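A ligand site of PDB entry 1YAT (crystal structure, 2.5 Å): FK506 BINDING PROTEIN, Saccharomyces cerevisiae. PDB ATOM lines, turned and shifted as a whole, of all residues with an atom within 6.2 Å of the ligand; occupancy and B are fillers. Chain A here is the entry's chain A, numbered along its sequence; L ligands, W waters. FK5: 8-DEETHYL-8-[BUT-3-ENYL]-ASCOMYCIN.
The side-chain carboxylate (OD2) of Asp 43 lies within hydrogen-bond range of an oxygen (O6) of the ligand (2.6 Å).
The side-chain hydroxyl (OH) of Tyr 88 lies within hydrogen-bond range of an oxygen (O3) of the ligand (2.6 Å).
O of Gln 60 lies within hydrogen-bond range of O10 of the ligand (2.8 Å).
An oxygen (O2) of the ligand sits at hydrogen-bond distance from the backbone NH (N) of Ile 62, 2.8 Å away.
OH of Tyr 32 is in hydrogen-bond range of OD2 of Asp 43, 2.7 Å away.
The side-chain carboxylate (OD1) of Asp 43 is in salt-bridge range of the guanidinium group (NH1) of Arg 48 (3.0 Å).
N of Gly 34 lies within hydrogen-bond range of O of Asp 43 (2.7 Å).
The guanidinium group (NH2) of Arg 48 lies within hydrogen-bond range of the side-chain hydroxyl (OH) of Tyr 32 (3.1 Å).
OG of Ser 44 sits at hydrogen-bond distance from O of Tyr 32, at 3.1 Å.
N of Phe 42 is in hydrogen-bond range of O of Gly 34 (2.9 Å).
The backbone carbonyl oxygen of Ser 44 lies within hydrogen-bond range of the guanidinium group of Arg 48 (3.3 Å).
Merely in contact with the ligand: Tyr 32, Phe 42, Arg 48, Phe 52, Val 61, Trp 65, Ala 87, Leu 96, Ile 97 and Phe 105.
Hydrophobic or aromatic side chains within 4 Å of the ligand: Tyr 32, Phe 42, Phe 52, Val 61, Ile 62, Trp 65, Tyr 88, Leu 96, Ile 97 and Phe 105.
14 residues have an atom within 4 Å of the ligand: Tyr 32, Phe 42, Asp 43, Arg 48, Phe 52, Gln 60, Val 61, Ile 62, Trp 65, Ala 87, Tyr 88, Leu 96, Ile 97 and Phe 105.
The nearest printed residue that does not touch the ligand is Phe 93 (4.1 Å).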
ATOM      1  N   TYR A  32     -24.002 -20.484 -10.065  1.00  0.00           N
ATOM      2  CA  TYR A  32     -24.752 -19.440 -10.730  1.00  0.00           C
ATOM      3  C   TYR A  32     -26.164 -19.326 -10.218  1.00  0.00           C
ATOM      4  O   TYR A  32     -26.674 -20.243  -9.616  1.00  0.00           O
ATOM      5  CB  TYR A  32     -24.728 -19.792 -12.266  1.00  0.00           C
ATOM      6  CG  TYR A  32     -25.551 -20.971 -12.670  1.00  0.00           C
ATOM      7  CD1 TYR A  32     -26.890 -20.799 -13.010  1.00  0.00           C
ATOM      8  CD2 TYR A  32     -25.017 -22.246 -12.834  1.00  0.00           C
ATOM      9  CE1 TYR A  32     -27.718 -21.838 -13.422  1.00  0.00           C
ATOM     10  CE2 TYR A  32     -25.825 -23.321 -13.263  1.00  0.00           C
ATOM     11  CZ  TYR A  32     -27.167 -23.094 -13.520  1.00  0.00           C
ATOM     12  OH  TYR A  32     -27.948 -24.175 -13.934  1.00  0.00           O
ATOM     13  N   GLY A  34     -29.657 -17.688 -12.169  1.00  0.00           N
ATOM     14  CA  GLY A  34     -30.145 -17.068 -13.399  1.00  0.00           C
ATOM     15  C   GLY A  34     -31.499 -16.445 -13.112  1.00  0.00           C
ATOM     16  O   GLY A  34     -32.440 -17.048 -12.569  1.00  0.00           O
ATOM     17  N   PHE A  42     -35.102 -18.138 -12.677  1.00  0.00           N
ATOM     18  CA  PHE A  42     -35.502 -19.328 -13.410  1.00  0.00           C
ATOM     19  C   PHE A  42     -34.610 -20.513 -13.114  1.00  0.00           C
ATOM     20  O   PHE A  42     -34.950 -21.654 -13.500  1.00  0.00           O
ATOM     21  CB  PHE A  42     -35.545 -19.049 -14.934  1.00  0.00           C
ATOM     22  CG  PHE A  42     -34.194 -18.736 -15.546  1.00  0.00           C
ATOM     23  CD1 PHE A  42     -33.291 -19.737 -15.816  1.00  0.00           C
ATOM     24  CD2 PHE A  42     -33.814 -17.405 -15.716  1.00  0.00           C
ATOM     25  CE1 PHE A  42     -32.003 -19.442 -16.341  1.00  0.00           C
ATOM     26  CE2 PHE A  42     -32.553 -17.045 -16.183  1.00  0.00           C
ATOM     27  CZ  PHE A  42     -31.673 -18.082 -16.503  1.00  0.00           C
ATOM     28  N   ASP A  43     -33.466 -20.341 -12.502  1.00  0.00           N
ATOM     29  CA  ASP A  43     -32.563 -21.479 -12.187  1.00  0.00           C
ATOM     30  C   ASP A  43     -31.448 -21.036 -11.284  1.00  0.00           C
ATOM     31  O   ASP A  43     -31.069 -19.873 -11.337  1.00  0.00           O
ATOM     32  CB  ASP A  43     -31.987 -22.069 -13.488  1.00  0.00           C
ATOM     33  CG  ASP A  43     -31.333 -23.400 -13.249  1.00  0.00           C
ATOM     34  OD1 ASP A  43     -31.498 -23.990 -12.165  1.00  0.00           O
ATOM     35  OD2 ASP A  43     -30.605 -23.934 -14.101  1.00  0.00           O
ATOM     36  N   SER A  44     -30.879 -21.939 -10.531  1.00  0.00           N
ATOM     37  CA  SER A  44     -29.772 -21.676  -9.625  1.00  0.00           C
ATOM     38  C   SER A  44     -29.106 -22.987  -9.289  1.00  0.00           C
ATOM     39  O   SER A  44     -29.877 -23.946  -9.105  1.00  0.00           O
ATOM     40  CB  SER A  44     -30.229 -21.066  -8.297  1.00  0.00           C
ATOM     41  OG  SER A  44     -28.953 -20.770  -7.620  1.00  0.00           O
ATOM     42  N   ARG A  48     -29.546 -26.343  -5.767  1.00  0.00           N
ATOM     43  CA  ARG A  48     -29.306 -27.745  -6.006  1.00  0.00           C
ATOM     44  C   ARG A  48     -28.193 -28.214  -5.064  1.00  0.00           C
ATOM     45  O   ARG A  48     -28.021 -29.420  -4.917  1.00  0.00           O
ATOM     46  CB  ARG A  48     -28.891 -28.102  -7.454  1.00  0.00           C
ATOM     47  CG  ARG A  48     -30.089 -28.203  -8.393  1.00  0.00           C
ATOM     48  CD  ARG A  48     -29.680 -28.874  -9.667  1.00  0.00           C
ATOM     49  NE  ARG A  48     -28.668 -28.075 -10.353  1.00  0.00           N
ATOM     50  CZ  ARG A  48     -29.059 -26.958 -11.032  1.00  0.00           C
ATOM     51  NH1 ARG A  48     -30.303 -26.513 -11.125  1.00  0.00           N
ATOM     52  NH2 ARG A  48     -28.087 -26.295 -11.688  1.00  0.00           N
ATOM     53  N   PHE A  52     -21.879 -26.146 -10.989  1.00  0.00           N
ATOM     54  CA  PHE A  52     -21.869 -26.534 -12.388  1.00  0.00           C
ATOM     55  C   PHE A  52     -20.413 -26.616 -12.901  1.00  0.00           C
ATOM     56  O   PHE A  52     -19.533 -25.847 -12.415  1.00  0.00           O
ATOM     57  CB  PHE A  52     -22.714 -25.580 -13.217  1.00  0.00           C
ATOM     58  CG  PHE A  52     -22.767 -25.747 -14.700  1.00  0.00           C
ATOM     59  CD1 PHE A  52     -23.402 -26.852 -15.269  1.00  0.00           C
ATOM     60  CD2 PHE A  52     -22.199 -24.801 -15.548  1.00  0.00           C
ATOM     61  CE1 PHE A  52     -23.495 -27.008 -16.660  1.00  0.00           C
ATOM     62  CE2 PHE A  52     -22.245 -24.946 -16.913  1.00  0.00           C
ATOM     63  CZ  PHE A  52     -22.899 -26.039 -17.483  1.00  0.00           C
ATOM     64  N   CYS A  54     -18.117 -27.277 -16.706  1.00  0.00           N
ATOM     65  CA  CYS A  54     -18.156 -27.329 -18.157  1.00  0.00           C
ATOM     66  C   CYS A  54     -16.727 -26.981 -18.596  1.00  0.00           C
ATOM     67  O   CYS A  54     -16.012 -26.479 -17.721  1.00  0.00           O
ATOM     68  CB  CYS A  54     -19.130 -26.385 -18.827  1.00  0.00           C
ATOM     69  SG  CYS A  54     -18.858 -24.614 -18.516  1.00  0.00           S
ATOM     70  N   GLY A  59     -18.123 -24.283 -27.048  1.00  0.00           N
ATOM     71  CA  GLY A  59     -19.519 -24.490 -27.423  1.00  0.00           C
ATOM     72  C   GLY A  59     -20.330 -25.399 -26.580  1.00  0.00           C
ATOM     73  O   GLY A  59     -21.361 -25.872 -27.092  1.00  0.00           O
ATOM     74  N   GLN A  60     -19.958 -25.666 -25.326  1.00  0.00           N
ATOM     75  CA  GLN A  60     -20.728 -26.478 -24.396  1.00  0.00           C
ATOM     76  C   GLN A  60     -21.855 -25.659 -23.800  1.00  0.00           C
ATOM     77  O   GLN A  60     -22.930 -26.257 -23.573  1.00  0.00           O
ATOM     78  CB  GLN A  60     -19.940 -27.140 -23.277  1.00  0.00           C
ATOM     79  CG  GLN A  60     -19.003 -28.271 -23.756  1.00  0.00           C
ATOM     80  CD  GLN A  60     -18.246 -28.867 -22.611  1.00  0.00           C
ATOM     81  OE1 GLN A  60     -17.386 -29.740 -22.729  1.00  0.00           O
ATOM     82  NE2 GLN A  60     -18.547 -28.460 -21.377  1.00  0.00           N
ATOM     83  N   VAL A  61     -21.711 -24.369 -23.621  1.00  0.00           N
ATOM     84  CA  VAL A  61     -22.740 -23.470 -23.016  1.00  0.00           C
ATOM     85  C   VAL A  61     -23.046 -22.315 -23.964  1.00  0.00           C
ATOM     86  O   VAL A  61     -22.348 -22.212 -25.010  1.00  0.00           O
ATOM     87  CB  VAL A  61     -22.144 -23.000 -21.672  1.00  0.00           C
ATOM     88  CG1 VAL A  61     -21.884 -24.151 -20.702  1.00  0.00           C
ATOM     89  CG2 VAL A  61     -20.863 -22.239 -21.922  1.00  0.00           C
ATOM     90  N   ILE A  62     -24.042 -21.530 -23.737  1.00  0.00           N
ATOM     91  CA  ILE A  62     -24.477 -20.371 -24.566  1.00  0.00           C
ATOM     92  C   ILE A  62     -23.250 -19.456 -24.647  1.00  0.00           C
ATOM     93  O   ILE A  62     -22.408 -19.487 -23.735  1.00  0.00           O
ATOM     94  CB  ILE A  62     -25.714 -19.683 -23.857  1.00  0.00           C
ATOM     95  CG1 ILE A  62     -25.304 -19.267 -22.438  1.00  0.00           C
ATOM     96  CG2 ILE A  62     -26.898 -20.659 -23.851  1.00  0.00           C
ATOM     97  CD1 ILE A  62     -26.291 -18.372 -21.607  1.00  0.00           C
ATOM     98  N   TRP A  65     -21.719 -17.116 -21.866  1.00  0.00           N
ATOM     99  CA  TRP A  65     -20.947 -17.824 -20.886  1.00  0.00           C
ATOM    100  C   TRP A  65     -19.522 -17.985 -21.476  1.00  0.00           C
ATOM    101  O   TRP A  65     -18.581 -17.775 -20.718  1.00  0.00           O
ATOM    102  CB  TRP A  65     -21.532 -19.169 -20.448  1.00  0.00           C
ATOM    103  CG  TRP A  65     -22.373 -19.046 -19.221  1.00  0.00           C
ATOM    104  CD1 TRP A  65     -23.471 -18.245 -19.036  1.00  0.00           C
ATOM    105  CD2 TRP A  65     -22.214 -19.786 -17.996  1.00  0.00           C
ATOM    106  NE1 TRP A  65     -23.974 -18.439 -17.797  1.00  0.00           N
ATOM    107  CE2 TRP A  65     -23.215 -19.351 -17.117  1.00  0.00           C
ATOM    108  CE3 TRP A  65     -21.276 -20.739 -17.577  1.00  0.00           C
ATOM    109  CZ2 TRP A  65     -23.335 -19.834 -15.823  1.00  0.00           C
ATOM    110  CZ3 TRP A  65     -21.394 -21.219 -16.293  1.00  0.00           C
ATOM    111  CH2 TRP A  65     -22.419 -20.784 -15.442  1.00  0.00           C
ATOM    112  N   ALA A  87     -27.443 -15.811 -25.937  1.00  0.00           N
ATOM    113  CA  ALA A  87     -28.173 -16.687 -25.073  1.00  0.00           C
ATOM    114  C   ALA A  87     -29.109 -17.602 -25.873  1.00  0.00           C
ATOM    115  O   ALA A  87     -28.564 -18.365 -26.697  1.00  0.00           O
ATOM    116  CB  ALA A  87     -28.976 -15.965 -23.992  1.00  0.00           C
ATOM    117  N   TYR A  88     -30.384 -17.543 -25.670  1.00  0.00           N
ATOM    118  CA  TYR A  88     -31.334 -18.462 -26.365  1.00  0.00           C
ATOM    119  C   TYR A  88     -32.051 -17.781 -27.514  1.00  0.00           C
ATOM    120  O   TYR A  88     -32.937 -18.398 -28.135  1.00  0.00           O
ATOM    121  CB  TYR A  88     -32.383 -19.069 -25.341  1.00  0.00           C
ATOM    122  CG  TYR A  88     -31.680 -19.950 -24.350  1.00  0.00           C
ATOM    123  CD1 TYR A  88     -31.355 -21.280 -24.618  1.00  0.00           C
ATOM    124  CD2 TYR A  88     -31.148 -19.395 -23.189  1.00  0.00           C
ATOM    125  CE1 TYR A  88     -30.623 -22.076 -23.722  1.00  0.00           C
ATOM    126  CE2 TYR A  88     -30.391 -20.139 -22.290  1.00  0.00           C
ATOM    127  CZ  TYR A  88     -30.150 -21.452 -22.542  1.00  0.00           C
ATOM    128  OH  TYR A  88     -29.363 -22.129 -21.656  1.00  0.00           O
ATOM    129  N   GLY A  89     -31.729 -16.519 -27.820  1.00  0.00           N
ATOM    130  CA  GLY A  89     -32.392 -15.840 -28.934  1.00  0.00           C
ATOM    131  C   GLY A  89     -33.917 -15.981 -28.939  1.00  0.00           C
ATOM    132  O   GLY A  89     -34.609 -16.002 -27.885  1.00  0.00           O
ATOM    133  N   PHE A  93     -36.325 -21.238 -24.056  1.00  0.00           N
ATOM    134  CA  PHE A  93     -36.258 -22.573 -23.403  1.00  0.00           C
ATOM    135  C   PHE A  93     -37.613 -22.816 -22.747  1.00  0.00           C
ATOM    136  O   PHE A  93     -38.148 -21.925 -22.051  1.00  0.00           O
ATOM    137  CB  PHE A  93     -35.058 -22.662 -22.463  1.00  0.00           C
ATOM    138  CG  PHE A  93     -34.761 -24.108 -22.147  1.00  0.00           C
ATOM    139  CD1 PHE A  93     -35.499 -24.772 -21.160  1.00  0.00           C
ATOM    140  CD2 PHE A  93     -33.826 -24.786 -22.929  1.00  0.00           C
ATOM    141  CE1 PHE A  93     -35.293 -26.122 -20.901  1.00  0.00           C
ATOM    142  CE2 PHE A  93     -33.603 -26.142 -22.657  1.00  0.00           C
ATOM    143  CZ  PHE A  93     -34.333 -26.781 -21.648  1.00  0.00           C
ATOM    144  N   LEU A  96     -38.894 -21.753 -19.121  1.00  0.00           N
ATOM    145  CA  LEU A  96     -37.902 -21.050 -18.291  1.00  0.00           C
ATOM    146  C   LEU A  96     -37.593 -19.653 -18.804  1.00  0.00           C
ATOM    147  O   LEU A  96     -37.540 -18.689 -18.041  1.00  0.00           O
ATOM    148  CB  LEU A  96     -36.645 -21.962 -18.223  1.00  0.00           C
ATOM    149  CG  LEU A  96     -36.657 -23.170 -17.352  1.00  0.00           C
ATOM    150  CD1 LEU A  96     -35.372 -23.921 -17.200  1.00  0.00           C
ATOM    151  CD2 LEU A  96     -37.047 -22.719 -15.931  1.00  0.00           C
ATOM    152  N   ILE A  97     -37.375 -19.626 -20.130  1.00  0.00           N
ATOM    153  CA  ILE A  97     -36.967 -18.444 -20.853  1.00  0.00           C
ATOM    154  C   ILE A  97     -37.682 -18.190 -22.146  1.00  0.00           C
ATOM    155  O   ILE A  97     -37.548 -19.022 -23.088  1.00  0.00           O
ATOM    156  CB  ILE A  97     -35.419 -18.801 -21.250  1.00  0.00           C
ATOM    157  CG1 ILE A  97     -34.640 -18.827 -19.918  1.00  0.00           C
ATOM    158  CG2 ILE A  97     -34.920 -17.800 -22.315  1.00  0.00           C
ATOM    159  CD1 ILE A  97     -33.389 -19.669 -19.838  1.00  0.00           C
ATOM    160  N   LEU A 103     -30.643 -12.350 -20.232  1.00  0.00           N
ATOM    161  CA  LEU A 103     -30.434 -13.125 -19.061  1.00  0.00           C
ATOM    162  C   LEU A 103     -29.423 -12.451 -18.149  1.00  0.00           C
ATOM    163  O   LEU A 103     -28.409 -11.912 -18.630  1.00  0.00           O
ATOM    164  CB  LEU A 103     -29.944 -14.537 -19.499  1.00  0.00           C
ATOM    165  CG  LEU A 103     -30.711 -15.376 -20.469  1.00  0.00           C
ATOM    166  CD1 LEU A 103     -30.293 -16.860 -20.570  1.00  0.00           C
ATOM    167  CD2 LEU A 103     -32.203 -15.329 -20.130  1.00  0.00           C
ATOM    168  N   PHE A 105     -26.903 -13.363 -14.997  1.00  0.00           N
ATOM    169  CA  PHE A 105     -26.270 -14.480 -14.299  1.00  0.00           C
ATOM    170  C   PHE A 105     -25.333 -13.932 -13.200  1.00  0.00           C
ATOM    171  O   PHE A 105     -24.447 -13.119 -13.458  1.00  0.00           O
ATOM    172  CB  PHE A 105     -25.542 -15.397 -15.270  1.00  0.00           C
ATOM    173  CG  PHE A 105     -26.369 -16.389 -16.035  1.00  0.00           C
ATOM    174  CD1 PHE A 105     -26.786 -17.597 -15.420  1.00  0.00           C
ATOM    175  CD2 PHE A 105     -26.665 -16.188 -17.379  1.00  0.00           C
ATOM    176  CE1 PHE A 105     -27.563 -18.512 -16.103  1.00  0.00           C
ATOM    177  CE2 PHE A 105     -27.443 -17.090 -18.101  1.00  0.00           C
ATOM    178  CZ  PHE A 105     -27.914 -18.245 -17.451  1.00  0.00           C
HETATM  179  C1  FK5 L   1     -26.105 -23.275 -20.697  1.00  0.00           C
HETATM  180  C2  FK5 L   1     -26.553 -22.280 -19.660  1.00  0.00           C
HETATM  181  C3  FK5 L   1     -25.283 -21.637 -19.041  1.00  0.00           C
HETATM  182  C4  FK5 L   1     -24.656 -22.674 -18.144  1.00  0.00           C
HETATM  183  C5  FK5 L   1     -25.498 -22.996 -16.915  1.00  0.00           C
HETATM  184  C6  FK5 L   1     -26.809 -23.555 -17.408  1.00  0.00           C
HETATM  185  C8  FK5 L   1     -28.581 -22.149 -18.366  1.00  0.00           C
HETATM  186  C9  FK5 L   1     -29.506 -22.452 -17.218  1.00  0.00           C
HETATM  187  C10 FK5 L   1     -30.545 -23.552 -17.411  1.00  0.00           C
HETATM  188  C11 FK5 L   1     -31.166 -23.682 -18.820  1.00  0.00           C
HETATM  189  C12 FK5 L   1     -31.920 -25.030 -18.829  1.00  0.00           C
HETATM  190  C13 FK5 L   1     -30.931 -26.201 -18.547  1.00  0.00           C
HETATM  191  C14 FK5 L   1     -30.399 -25.946 -17.096  1.00  0.00           C
HETATM  192  C15 FK5 L   1     -29.460 -26.901 -16.363  1.00  0.00           C
HETATM  193  C16 FK5 L   1     -28.253 -27.420 -17.098  1.00  0.00           C
HETATM  194  C17 FK5 L   1     -27.176 -28.233 -16.325  1.00  0.00           C
HETATM  195  C18 FK5 L   1     -27.416 -29.739 -16.483  1.00  0.00           C
HETATM  196  C19 FK5 L   1     -27.155 -30.329 -17.799  1.00  0.00           C
HETATM  197  C20 FK5 L   1     -28.193 -30.442 -18.680  1.00  0.00           C
HETATM  198  C21 FK5 L   1     -28.028 -30.907 -20.110  1.00  0.00           C
HETATM  199  C22 FK5 L   1     -27.807 -29.739 -21.060  1.00  0.00           C
HETATM  200  C23 FK5 L   1     -26.393 -29.411 -21.443  1.00  0.00           C
HETATM  201  C24 FK5 L   1     -26.191 -28.032 -21.990  1.00  0.00           C
HETATM  202  C25 FK5 L   1     -26.399 -26.897 -20.910  1.00  0.00           C
HETATM  203  C26 FK5 L   1     -26.411 -25.476 -21.541  1.00  0.00           C
HETATM  204  C27 FK5 L   1     -27.454 -25.246 -22.622  1.00  0.00           C
HETATM  205  C28 FK5 L   1     -26.955 -25.039 -23.836  1.00  0.00           C
HETATM  206  C29 FK5 L   1     -27.739 -24.951 -25.072  1.00  0.00           C
HETATM  207  C30 FK5 L   1     -27.600 -23.680 -25.889  1.00  0.00           C
HETATM  208  C31 FK5 L   1     -28.393 -23.755 -27.204  1.00  0.00           C
HETATM  209  C32 FK5 L   1     -27.901 -24.968 -27.977  1.00  0.00           C
HETATM  210  C33 FK5 L   1     -27.905 -26.258 -27.175  1.00  0.00           C
HETATM  211  C34 FK5 L   1     -27.024 -26.066 -25.928  1.00  0.00           C
HETATM  212  C35 FK5 L   1     -32.133 -22.578 -19.184  1.00  0.00           C
HETATM  213  C36 FK5 L   1     -27.169 -27.947 -14.814  1.00  0.00           C
HETATM  214  C37 FK5 L   1     -25.726 -30.764 -18.112  1.00  0.00           C
HETATM  215  C38 FK5 L   1     -29.315 -31.733 -20.502  1.00  0.00           C
HETATM  216  C39 FK5 L   1     -28.893 -32.877 -21.443  1.00  0.00           C
HETATM  217  C40 FK5 L   1     -29.361 -32.890 -22.708  1.00  0.00           C
HETATM  218  C41 FK5 L   1     -25.199 -26.857 -19.915  1.00  0.00           C
HETATM  219  C42 FK5 L   1     -28.929 -25.546 -22.320  1.00  0.00           C
HETATM  220  C43 FK5 L   1     -31.019 -28.527 -19.313  1.00  0.00           C
HETATM  221  C44 FK5 L   1     -30.366 -28.150 -14.552  1.00  0.00           C
HETATM  222  C45 FK5 L   1     -28.925 -21.466 -27.718  1.00  0.00           C
HETATM  223  N7  FK5 L   1     -27.361 -22.709 -18.492  1.00  0.00           N
HETATM  224  O1  FK5 L   1     -26.580 -24.516 -20.477  1.00  0.00           O
HETATM  225  O2  FK5 L   1     -25.428 -22.955 -21.696  1.00  0.00           O
HETATM  226  O3  FK5 L   1     -29.016 -21.327 -19.199  1.00  0.00           O
HETATM  227  O4  FK5 L   1     -29.415 -21.737 -16.224  1.00  0.00           O
HETATM  228  O5  FK5 L   1     -29.694 -24.694 -17.144  1.00  0.00           O
HETATM  229  O6  FK5 L   1     -31.569 -23.513 -16.455  1.00  0.00           O
HETATM  230  O7  FK5 L   1     -31.667 -27.447 -18.636  1.00  0.00           O
HETATM  231  O8  FK5 L   1     -30.375 -27.964 -15.991  1.00  0.00           O
HETATM  232  O9  FK5 L   1     -28.785 -29.057 -21.460  1.00  0.00           O
HETATM  233  O10 FK5 L   1     -24.776 -27.974 -22.356  1.00  0.00           O
HETATM  234  O11 FK5 L   1     -28.161 -22.615 -28.074  1.00  0.00           O
HETATM  235  O12 FK5 L   1     -28.817 -25.045 -29.064  1.00  0.00           O
HETATM  236  O   HOH W   1     -28.748 -33.402 -25.875  1.00  0.00           O
